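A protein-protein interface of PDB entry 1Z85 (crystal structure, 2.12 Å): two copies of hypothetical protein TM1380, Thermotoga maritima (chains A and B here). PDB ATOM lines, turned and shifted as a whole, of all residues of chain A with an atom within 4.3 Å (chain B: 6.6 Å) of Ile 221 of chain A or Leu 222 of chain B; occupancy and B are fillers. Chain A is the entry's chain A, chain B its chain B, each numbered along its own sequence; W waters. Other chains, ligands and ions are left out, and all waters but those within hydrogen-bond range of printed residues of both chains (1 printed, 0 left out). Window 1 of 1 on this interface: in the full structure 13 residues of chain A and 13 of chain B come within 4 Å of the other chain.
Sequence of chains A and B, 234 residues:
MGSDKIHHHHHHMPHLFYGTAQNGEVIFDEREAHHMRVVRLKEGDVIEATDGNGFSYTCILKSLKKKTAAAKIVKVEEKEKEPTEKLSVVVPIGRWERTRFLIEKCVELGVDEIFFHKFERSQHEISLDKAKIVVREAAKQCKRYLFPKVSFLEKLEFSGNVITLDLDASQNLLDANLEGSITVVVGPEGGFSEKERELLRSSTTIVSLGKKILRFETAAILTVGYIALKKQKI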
ATOM      1  N   PHE A 101     -14.048  -1.956  -0.484  1.00  0.00           N
ATOM      2  CA  PHE A 101     -14.495  -3.244  -1.040  1.00  0.00           C
ATOM      3  C   PHE A 101     -13.564  -4.411  -0.666  1.00  0.00           C
ATOM      4  O   PHE A 101     -14.001  -5.471  -0.169  1.00  0.00           O
ATOM      5  CB  PHE A 101     -14.659  -3.121  -2.547  1.00  0.00           C
ATOM      6  CG  PHE A 101     -15.108  -4.359  -3.184  1.00  0.00           C
ATOM      7  CD1 PHE A 101     -16.459  -4.676  -3.235  1.00  0.00           C
ATOM      8  CD2 PHE A 101     -14.195  -5.224  -3.740  1.00  0.00           C
ATOM      9  CE1 PHE A 101     -16.864  -5.857  -3.831  1.00  0.00           C
ATOM     10  CE2 PHE A 101     -14.616  -6.419  -4.345  1.00  0.00           C
ATOM     11  CZ  PHE A 101     -15.918  -6.709  -4.396  1.00  0.00           C
ATOM     12  N   LYS A 105     -14.514  -7.768   1.553  1.00  0.00           N
ATOM     13  CA  LYS A 105     -14.328  -9.099   1.032  1.00  0.00           C
ATOM     14  C   LYS A 105     -13.386  -9.895   1.886  1.00  0.00           C
ATOM     15  O   LYS A 105     -13.613 -11.049   2.097  1.00  0.00           O
ATOM     16  CB  LYS A 105     -13.797  -9.043  -0.420  1.00  0.00           C
ATOM     17  CG  LYS A 105     -14.761  -8.502  -1.459  1.00  0.00           C
ATOM     18  CD  LYS A 105     -16.230  -9.021  -1.379  1.00  0.00           C
ATOM     19  CE  LYS A 105     -17.105  -7.993  -0.740  1.00  0.00           C
ATOM     20  NZ  LYS A 105     -18.546  -8.240  -0.928  1.00  0.00           N
ATOM     21  N   GLU A 217     -14.128  -5.806  -9.092  1.00  0.00           N
ATOM     22  CA  GLU A 217     -14.860  -6.424  -8.011  1.00  0.00           C
ATOM     23  C   GLU A 217     -15.127  -7.890  -8.241  1.00  0.00           C
ATOM     24  O   GLU A 217     -15.051  -8.691  -7.302  1.00  0.00           O
ATOM     25  CB  GLU A 217     -16.187  -5.706  -7.775  1.00  0.00           C
ATOM     26  CG  GLU A 217     -15.992  -4.316  -7.227  1.00  0.00           C
ATOM     27  CD  GLU A 217     -17.259  -3.694  -6.668  1.00  0.00           C
ATOM     28  OE1 GLU A 217     -18.341  -4.326  -6.741  1.00  0.00           O
ATOM     29  OE2 GLU A 217     -17.169  -2.560  -6.119  1.00  0.00           O
ATOM     30  N   THR A 218     -15.466  -8.235  -9.483  1.00  0.00           N
ATOM     31  CA  THR A 218     -15.617  -9.631  -9.926  1.00  0.00           C
ATOM     32  C   THR A 218     -14.303 -10.446  -9.751  1.00  0.00           C
ATOM     33  O   THR A 218     -14.279 -11.546  -9.175  1.00  0.00           O
ATOM     34  CB  THR A 218     -16.094  -9.652 -11.399  1.00  0.00           C
ATOM     35  OG1 THR A 218     -17.191  -8.721 -11.556  1.00  0.00           O
ATOM     36  CG2 THR A 218     -16.572 -11.027 -11.798  1.00  0.00           C
ATOM     37  N   ALA A 219     -13.216  -9.892 -10.256  1.00  0.00           N
ATOM     38  CA  ALA A 219     -11.871 -10.465 -10.125  1.00  0.00           C
ATOM     39  C   ALA A 219     -11.415 -10.637  -8.708  1.00  0.00           C
ATOM     40  O   ALA A 219     -10.671 -11.542  -8.391  1.00  0.00           O
ATOM     41  CB  ALA A 219     -10.849  -9.528 -10.857  1.00  0.00           C
ATOM     42  N   ALA A 220     -11.752  -9.679  -7.855  1.00  0.00           N
ATOM     43  CA  ALA A 220     -11.290  -9.709  -6.493  1.00  0.00           C
ATOM     44  C   ALA A 220     -11.978 -10.839  -5.737  1.00  0.00           C
ATOM     45  O   ALA A 220     -11.346 -11.580  -5.014  1.00  0.00           O
ATOM     46  CB  ALA A 220     -11.555  -8.353  -5.833  1.00  0.00           C
ATOM     47  N   ILE A 221     -13.276 -10.971  -5.940  1.00  0.00           N
ATOM     48  CA  ILE A 221     -14.098 -12.029  -5.329  1.00  0.00           C
ATOM     49  C   ILE A 221     -13.735 -13.426  -5.846  1.00  0.00           C
ATOM     50  O   ILE A 221     -13.591 -14.388  -5.097  1.00  0.00           O
ATOM     51  CB  ILE A 221     -15.591 -11.765  -5.648  1.00  0.00           C
ATOM     52  CG1 ILE A 221     -16.095 -10.551  -4.880  1.00  0.00           C
ATOM     53  CG2 ILE A 221     -16.488 -13.013  -5.348  1.00  0.00           C
ATOM     54  CD1 ILE A 221     -17.510 -10.069  -5.314  1.00  0.00           C
ATOM     55  N   LEU A 222     -13.624 -13.554  -7.144  1.00  0.00           N
ATOM     56  CA  LEU A 222     -13.275 -14.827  -7.722  1.00  0.00           C
ATOM     57  C   LEU A 222     -11.915 -15.274  -7.234  1.00  0.00           C
ATOM     58  O   LEU A 222     -11.720 -16.415  -6.929  1.00  0.00           O
ATOM     59  CB  LEU A 222     -13.281 -14.688  -9.232  1.00  0.00           C
ATOM     60  CG  LEU A 222     -12.980 -15.835 -10.119  1.00  0.00           C
ATOM     61  CD1 LEU A 222     -13.957 -17.005  -9.748  1.00  0.00           C
ATOM     62  CD2 LEU A 222     -13.106 -15.355 -11.589  1.00  0.00           C
ATOM     63  N   THR A 223     -10.951 -14.373  -7.133  1.00  0.00           N
ATOM     64  CA  THR A 223      -9.601 -14.781  -6.782  1.00  0.00           C
ATOM     65  C   THR A 223      -9.419 -15.071  -5.297  1.00  0.00           C
ATOM     66  O   THR A 223      -8.992 -16.128  -4.930  1.00  0.00           O
ATOM     67  CB  THR A 223      -8.618 -13.639  -7.161  1.00  0.00           C
ATOM     68  OG1 THR A 223      -8.718 -13.369  -8.560  1.00  0.00           O
ATOM     69  CG2 THR A 223      -7.227 -14.034  -6.833  1.00  0.00           C
ATOM     70  N   VAL A 224      -9.708 -14.100  -4.434  1.00  0.00           N
ATOM     71  CA  VAL A 224      -9.677 -14.344  -3.001  1.00  0.00           C
ATOM     72  C   VAL A 224     -10.658 -15.410  -2.563  1.00  0.00           C
ATOM     73  O   VAL A 224     -10.377 -16.173  -1.671  1.00  0.00           O
ATOM     74  CB  VAL A 224      -9.980 -13.109  -2.275  1.00  0.00           C
ATOM     75  CG1 VAL A 224      -9.924 -13.346  -0.759  1.00  0.00           C
ATOM     76  CG2 VAL A 224      -8.940 -12.013  -2.673  1.00  0.00           C
ATOM     77  N   GLY A 225     -11.835 -15.462  -3.176  1.00  0.00           N
ATOM     78  CA  GLY A 225     -12.772 -16.518  -2.872  1.00  0.00           C
ATOM     79  C   GLY A 225     -12.326 -17.925  -3.207  1.00  0.00           C
ATOM     80  O   GLY A 225     -12.667 -18.868  -2.508  1.00  0.00           O
ATOM     81  N   TYR A 226     -11.683 -18.077  -4.354  1.00  0.00           N
ATOM     82  CA  TYR A 226     -11.173 -19.364  -4.764  1.00  0.00           C
ATOM     83  C   TYR A 226     -10.128 -19.818  -3.764  1.00  0.00           C
ATOM     84  O   TYR A 226     -10.148 -20.938  -3.318  1.00  0.00           O
ATOM     85  CB  TYR A 226     -10.535 -19.276  -6.151  1.00  0.00           C
ATOM     86  CG  TYR A 226      -9.835 -20.559  -6.479  1.00  0.00           C
ATOM     87  CD1 TYR A 226     -10.560 -21.735  -6.619  1.00  0.00           C
ATOM     88  CD2 TYR A 226      -8.435 -20.623  -6.545  1.00  0.00           C
ATOM     89  CE1 TYR A 226      -9.936 -22.932  -6.851  1.00  0.00           C
ATOM     90  CE2 TYR A 226      -7.797 -21.824  -6.816  1.00  0.00           C
ATOM     91  CZ  TYR A 226      -8.560 -22.974  -6.960  1.00  0.00           C
ATOM     92  OH  TYR A 226      -7.945 -24.175  -7.227  1.00  0.00           O
ATOM     93  N   ILE A 234     -13.865 -20.734   3.920  1.00  0.00           N
ATOM     94  CA  ILE A 234     -15.297 -20.589   3.718  1.00  0.00           C
ATOM     95  C   ILE A 234     -15.848 -21.924   3.190  1.00  0.00           C
ATOM     96  O   ILE A 234     -15.112 -22.790   2.685  1.00  0.00           O
ATOM     97  CB  ILE A 234     -15.684 -19.480   2.701  1.00  0.00           C
ATOM     98  CG1 ILE A 234     -15.112 -19.767   1.313  1.00  0.00           C
ATOM     99  CG2 ILE A 234     -15.251 -18.134   3.191  1.00  0.00           C
ATOM    100  CD1 ILE A 234     -15.308 -18.644   0.345  1.00  0.00           C
ATOM    101  OXT ILE A 234     -17.070 -22.094   3.251  1.00  0.00           O
ATOM    102  N   LEU B 109     -18.733 -13.260 -17.298  1.00  0.00           N
ATOM    103  CA  LEU B 109     -18.067 -14.529 -17.034  1.00  0.00           C
ATOM    104  C   LEU B 109     -18.109 -15.508 -18.192  1.00  0.00           C
ATOM    105  O   LEU B 109     -17.884 -16.723 -18.010  1.00  0.00           O
ATOM    106  CB  LEU B 109     -18.693 -15.212 -15.791  1.00  0.00           C
ATOM    107  CG  LEU B 109     -18.525 -14.381 -14.498  1.00  0.00           C
ATOM    108  CD1 LEU B 109     -19.312 -14.944 -13.344  1.00  0.00           C
ATOM    109  CD2 LEU B 109     -17.053 -14.277 -14.138  1.00  0.00           C
ATOM    110  N   LEU B 173     -18.204 -27.431  -4.294  1.00  0.00           N
ATOM    111  CA  LEU B 173     -18.027 -26.987  -5.665  1.00  0.00           C
ATOM    112  C   LEU B 173     -16.786 -27.576  -6.271  1.00  0.00           C
ATOM    113  O   LEU B 173     -16.794 -28.001  -7.409  1.00  0.00           O
ATOM    114  CB  LEU B 173     -17.926 -25.458  -5.700  1.00  0.00           C
ATOM    115  CG  LEU B 173     -17.762 -24.754  -7.056  1.00  0.00           C
ATOM    116  CD1 LEU B 173     -18.978 -24.942  -7.948  1.00  0.00           C
ATOM    117  CD2 LEU B 173     -17.479 -23.282  -6.836  1.00  0.00           C
ATOM    118  N   LEU B 214     -22.667 -17.926   1.982  1.00  0.00           N
ATOM    119  CA  LEU B 214     -22.234 -16.584   1.531  1.00  0.00           C
ATOM    120  C   LEU B 214     -23.380 -15.671   1.051  1.00  0.00           C
ATOM    121  O   LEU B 214     -24.434 -16.153   0.671  1.00  0.00           O
ATOM    122  CB  LEU B 214     -21.239 -16.713   0.371  1.00  0.00           C
ATOM    123  CG  LEU B 214     -19.829 -17.191   0.689  1.00  0.00           C
ATOM    124  CD1 LEU B 214     -19.137 -17.549  -0.635  1.00  0.00           C
ATOM    125  CD2 LEU B 214     -19.041 -16.152   1.552  1.00  0.00           C
ATOM    126  N   GLU B 217     -24.526 -12.324  -3.953  1.00  0.00           N
ATOM    127  CA  GLU B 217     -23.705 -11.847  -5.071  1.00  0.00           C
ATOM    128  C   GLU B 217     -22.347 -12.518  -5.108  1.00  0.00           C
ATOM    129  O   GLU B 217     -21.796 -12.803  -6.172  1.00  0.00           O
ATOM    130  CB  GLU B 217     -23.557 -10.326  -5.012  1.00  0.00           C
ATOM    131  CG  GLU B 217     -24.866  -9.526  -5.324  1.00  0.00           C
ATOM    132  CD  GLU B 217     -24.631  -8.004  -5.570  1.00  0.00           C
ATOM    133  OE1 GLU B 217     -23.450  -7.518  -5.480  1.00  0.00           O
ATOM    134  OE2 GLU B 217     -25.643  -7.307  -5.890  1.00  0.00           O
ATOM    135  N   THR B 218     -21.802 -12.803  -3.937  1.00  0.00           N
ATOM    136  CA  THR B 218     -20.501 -13.491  -3.833  1.00  0.00           C
ATOM    137  C   THR B 218     -20.578 -14.964  -4.245  1.00  0.00           C
ATOM    138  O   THR B 218     -19.750 -15.451  -5.043  1.00  0.00           O
ATOM    139  CB  THR B 218     -19.946 -13.317  -2.410  1.00  0.00           C
ATOM    140  OG1 THR B 218     -19.846 -11.924  -2.134  1.00  0.00           O
ATOM    141  CG2 THR B 218     -18.566 -13.912  -2.259  1.00  0.00           C
ATOM    142  N   ALA B 219     -21.554 -15.685  -3.711  1.00  0.00           N
ATOM    143  CA  ALA B 219     -21.768 -17.089  -4.105  1.00  0.00           C
ATOM    144  C   ALA B 219     -21.956 -17.273  -5.611  1.00  0.00           C
ATOM    145  O   ALA B 219     -21.488 -18.259  -6.179  1.00  0.00           O
ATOM    146  CB  ALA B 219     -22.987 -17.656  -3.414  1.00  0.00           C
ATOM    147  N   ALA B 220     -22.723 -16.376  -6.240  1.00  0.00           N
ATOM    148  CA  ALA B 220     -22.998 -16.477  -7.674  1.00  0.00           C
ATOM    149  C   ALA B 220     -21.758 -16.220  -8.528  1.00  0.00           C
ATOM    150  O   ALA B 220     -21.510 -16.900  -9.504  1.00  0.00           O
ATOM    151  CB  ALA B 220     -24.050 -15.504  -8.034  1.00  0.00           C
ATOM    152  N   ILE B 221     -20.967 -15.231  -8.127  1.00  0.00           N
ATOM    153  CA  ILE B 221     -19.719 -14.925  -8.837  1.00  0.00           C
ATOM    154  C   ILE B 221     -18.741 -16.036  -8.676  1.00  0.00           C
ATOM    155  O   ILE B 221     -18.088 -16.461  -9.623  1.00  0.00           O
ATOM    156  CB  ILE B 221     -19.112 -13.585  -8.303  1.00  0.00           C
ATOM    157  CG1 ILE B 221     -19.950 -12.401  -8.844  1.00  0.00           C
ATOM    158  CG2 ILE B 221     -17.668 -13.472  -8.658  1.00  0.00           C
ATOM    159  CD1 ILE B 221     -19.680 -11.063  -8.203  1.00  0.00           C
ATOM    160  N   LEU B 222     -18.587 -16.490  -7.439  1.00  0.00           N
ATOM    161  CA  LEU B 222     -17.631 -17.534  -7.155  1.00  0.00           C
ATOM    162  C   LEU B 222     -17.999 -18.842  -7.866  1.00  0.00           C
ATOM    163  O   LEU B 222     -17.148 -19.537  -8.438  1.00  0.00           O
ATOM    164  CB  LEU B 222     -17.544 -17.722  -5.656  1.00  0.00           C
ATOM    165  CG  LEU B 222     -16.347 -18.482  -5.168  1.00  0.00           C
ATOM    166  CD1 LEU B 222     -15.065 -17.749  -5.562  1.00  0.00           C
ATOM    167  CD2 LEU B 222     -16.523 -18.639  -3.662  1.00  0.00           C
ATOM    168  N   THR B 223     -19.269 -19.174  -7.854  1.00  0.00           N
ATOM    169  CA  THR B 223     -19.725 -20.442  -8.454  1.00  0.00           C
ATOM    170  C   THR B 223     -19.615 -20.449  -9.958  1.00  0.00           C
ATOM    171  O   THR B 223     -18.983 -21.318 -10.534  1.00  0.00           O
ATOM    172  CB  THR B 223     -21.163 -20.736  -8.019  1.00  0.00           C
ATOM    173  OG1 THR B 223     -21.186 -20.877  -6.598  1.00  0.00           O
ATOM    174  CG2 THR B 223     -21.669 -22.003  -8.661  1.00  0.00           C
ATOM    175  N   VAL B 224     -20.246 -19.484 -10.604  1.00  0.00           N
ATOM    176  CA  VAL B 224     -20.244 -19.423 -12.059  1.00  0.00           C
ATOM    177  C   VAL B 224     -18.860 -19.073 -12.551  1.00  0.00           C
ATOM    178  O   VAL B 224     -18.408 -19.537 -13.589  1.00  0.00           O
ATOM    179  CB  VAL B 224     -21.257 -18.363 -12.531  1.00  0.00           C
ATOM    180  CG1 VAL B 224     -21.225 -18.179 -14.064  1.00  0.00           C
ATOM    181  CG2 VAL B 224     -22.629 -18.717 -12.055  1.00  0.00           C
ATOM    182  N   GLY B 225     -18.175 -18.229 -11.810  1.00  0.00           N
ATOM    183  CA  GLY B 225     -16.822 -17.808 -12.173  1.00  0.00           C
ATOM    184  C   GLY B 225     -15.758 -18.869 -12.081  1.00  0.00           C
ATOM    185  O   GLY B 225     -14.865 -18.933 -12.938  1.00  0.00           O
ATOM    186  N   TYR B 226     -15.836 -19.714 -11.054  1.00  0.00           N
ATOM    187  CA  TYR B 226     -14.951 -20.864 -10.967  1.00  0.00           C
ATOM    188  C   TYR B 226     -15.168 -21.828 -12.132  1.00  0.00           C
ATOM    189  O   TYR B 226     -14.224 -22.327 -12.737  1.00  0.00           O
ATOM    190  CB  TYR B 226     -15.188 -21.610  -9.668  1.00  0.00           C
ATOM    191  CG  TYR B 226     -14.503 -22.971  -9.617  1.00  0.00           C
ATOM    192  CD1 TYR B 226     -13.102 -23.089  -9.510  1.00  0.00           C
ATOM    193  CD2 TYR B 226     -15.243 -24.130  -9.698  1.00  0.00           C
ATOM    194  CE1 TYR B 226     -12.481 -24.343  -9.472  1.00  0.00           C
ATOM    195  CE2 TYR B 226     -14.641 -25.375  -9.640  1.00  0.00           C
ATOM    196  CZ  TYR B 226     -13.278 -25.482  -9.534  1.00  0.00           C
ATOM    197  OH  TYR B 226     -12.728 -26.748  -9.499  1.00  0.00           O
ATOM    198  N   ILE B 227     -16.428 -22.134 -12.400  1.00  0.00           N
ATOM    199  CA  ILE B 227     -16.775 -22.992 -13.498  1.00  0.00           C
ATOM    200  C   ILE B 227     -16.282 -22.416 -14.848  1.00  0.00           C
ATOM    201  O   ILE B 227     -15.689 -23.105 -15.630  1.00  0.00           O
ATOM    202  CB  ILE B 227     -18.312 -23.276 -13.491  1.00  0.00           C
ATOM    203  CG1 ILE B 227     -18.664 -24.219 -12.317  1.00  0.00           C
ATOM    204  CG2 ILE B 227     -18.736 -23.901 -14.835  1.00  0.00           C
ATOM    205  CD1 ILE B 227     -20.106 -24.185 -11.808  1.00  0.00           C
HETATM  206  O   HOH W   1     -20.244  -9.460  -2.982  1.00  0.00           O
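Thr 218 of chain A touches Ile 221 of chain B, and with the chains exchanged Ile 221 of chain A touches Thr 218 of chain B.
Ile 221 of chain A touches its own counterpart, Ile 221 of chain B.
Leu 222 of chain A touches its own counterpart, Leu 222 of chain B.
Leu 222 of chain A touches Gly 225 of chain B, and with the chains exchanged Gly 225 of chain A touches Leu 222 of chain B.
Positions printed for both chains: 217, 218, 219, 220, 221, 222, 223, 224, 225 and 226.
Of the 10 pairs that touch across the chains among the printed residues, 9 have their exchanged pair printed and touching as well.
O of Thr 218 of chain A touches CG2 of Ile 221 of chain B, at 3.9 Å.
CG2 of Thr 218 of chain B touches CG2 of Ile 221 of chain A, at 3.8 Å.
Ile 221 of chain A touches Ile 221 of chain B (CG2 to CG2, 3.5 Å).
Ile 221 of chain A touches Leu 222 of chain B.
Leu 222 of chain A touches Leu 222 of chain B (O to CD1, 3.9 Å).
Gly 225 of chain B touches Leu 222 of chain A.
Leu 222 of chain A touches Tyr 226 of chain B.
Gly 225 of chain A touches Leu 222 of chain B.
Tyr 226 of chain A touches Leu 222 of chain B (N to CD1, 3.6 Å).
CE1 of Tyr 226 of chain A touches CE1 of Tyr 226 of chain B, at 3.9 Å.
Water W1 lies within hydrogen-bond range of OG1 of Thr 218 of chain B (2.6 Å) and NZ of Lys 105 of chain A (2.9 Å).
Printed residues of chain B that touch a printed residue of chain A: Thr 218, Ile 221, Leu 222, Gly 225 and Tyr 226.
Hydrophobic or aromatic side chains of chain B within 4 Å of the printed part of chain A: Ile 221, Leu 222 and Tyr 226.
Of the 13 printed residues of chain A, 5 touch a printed residue of chain B.
Hydrophobic or aromatic side chains of chain A within 4 Å of the printed part of chain B: Ile 221, Leu 222 and Tyr 226.
Among the printed residues, 10 pairs touch across the chains.
Among the printed residues, no Asp or Glu carboxylate lies within 4 Å of a Lys or Arg side-chain nitrogen of the other chain.
Of chain B, only Thr 218 (3.8 Å), Ile 221 (3.5 Å) and Leu 222 (3.7 Å) come within 4 Å of Ile 221 of chain A.
Leu 222 of chain B touches four residues of chain A.
Of the printed residues of chain A, Thr 218 of chain B touches Ile 221 (3.8 Å).
Printed residues of chain B within 4 Å of Tyr 226 of chain A: Leu 222 (3.6 Å) and Tyr 226 (3.9 Å).
Printed residues of chain B within 4 Å of Leu 222 of chain A: Leu 222 (3.9 Å), Gly 225 (3.5 Å) and Tyr 226 (3.5 Å).
Lys 105 of chain A touches none of the printed residues of chain B.
Glu 217 of chain B touches none of the printed residues of chain A.
The nearest printed residue of chain B that does not touch Thr 218 of chain A is Leu 109 of chain B (4.03 Å).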
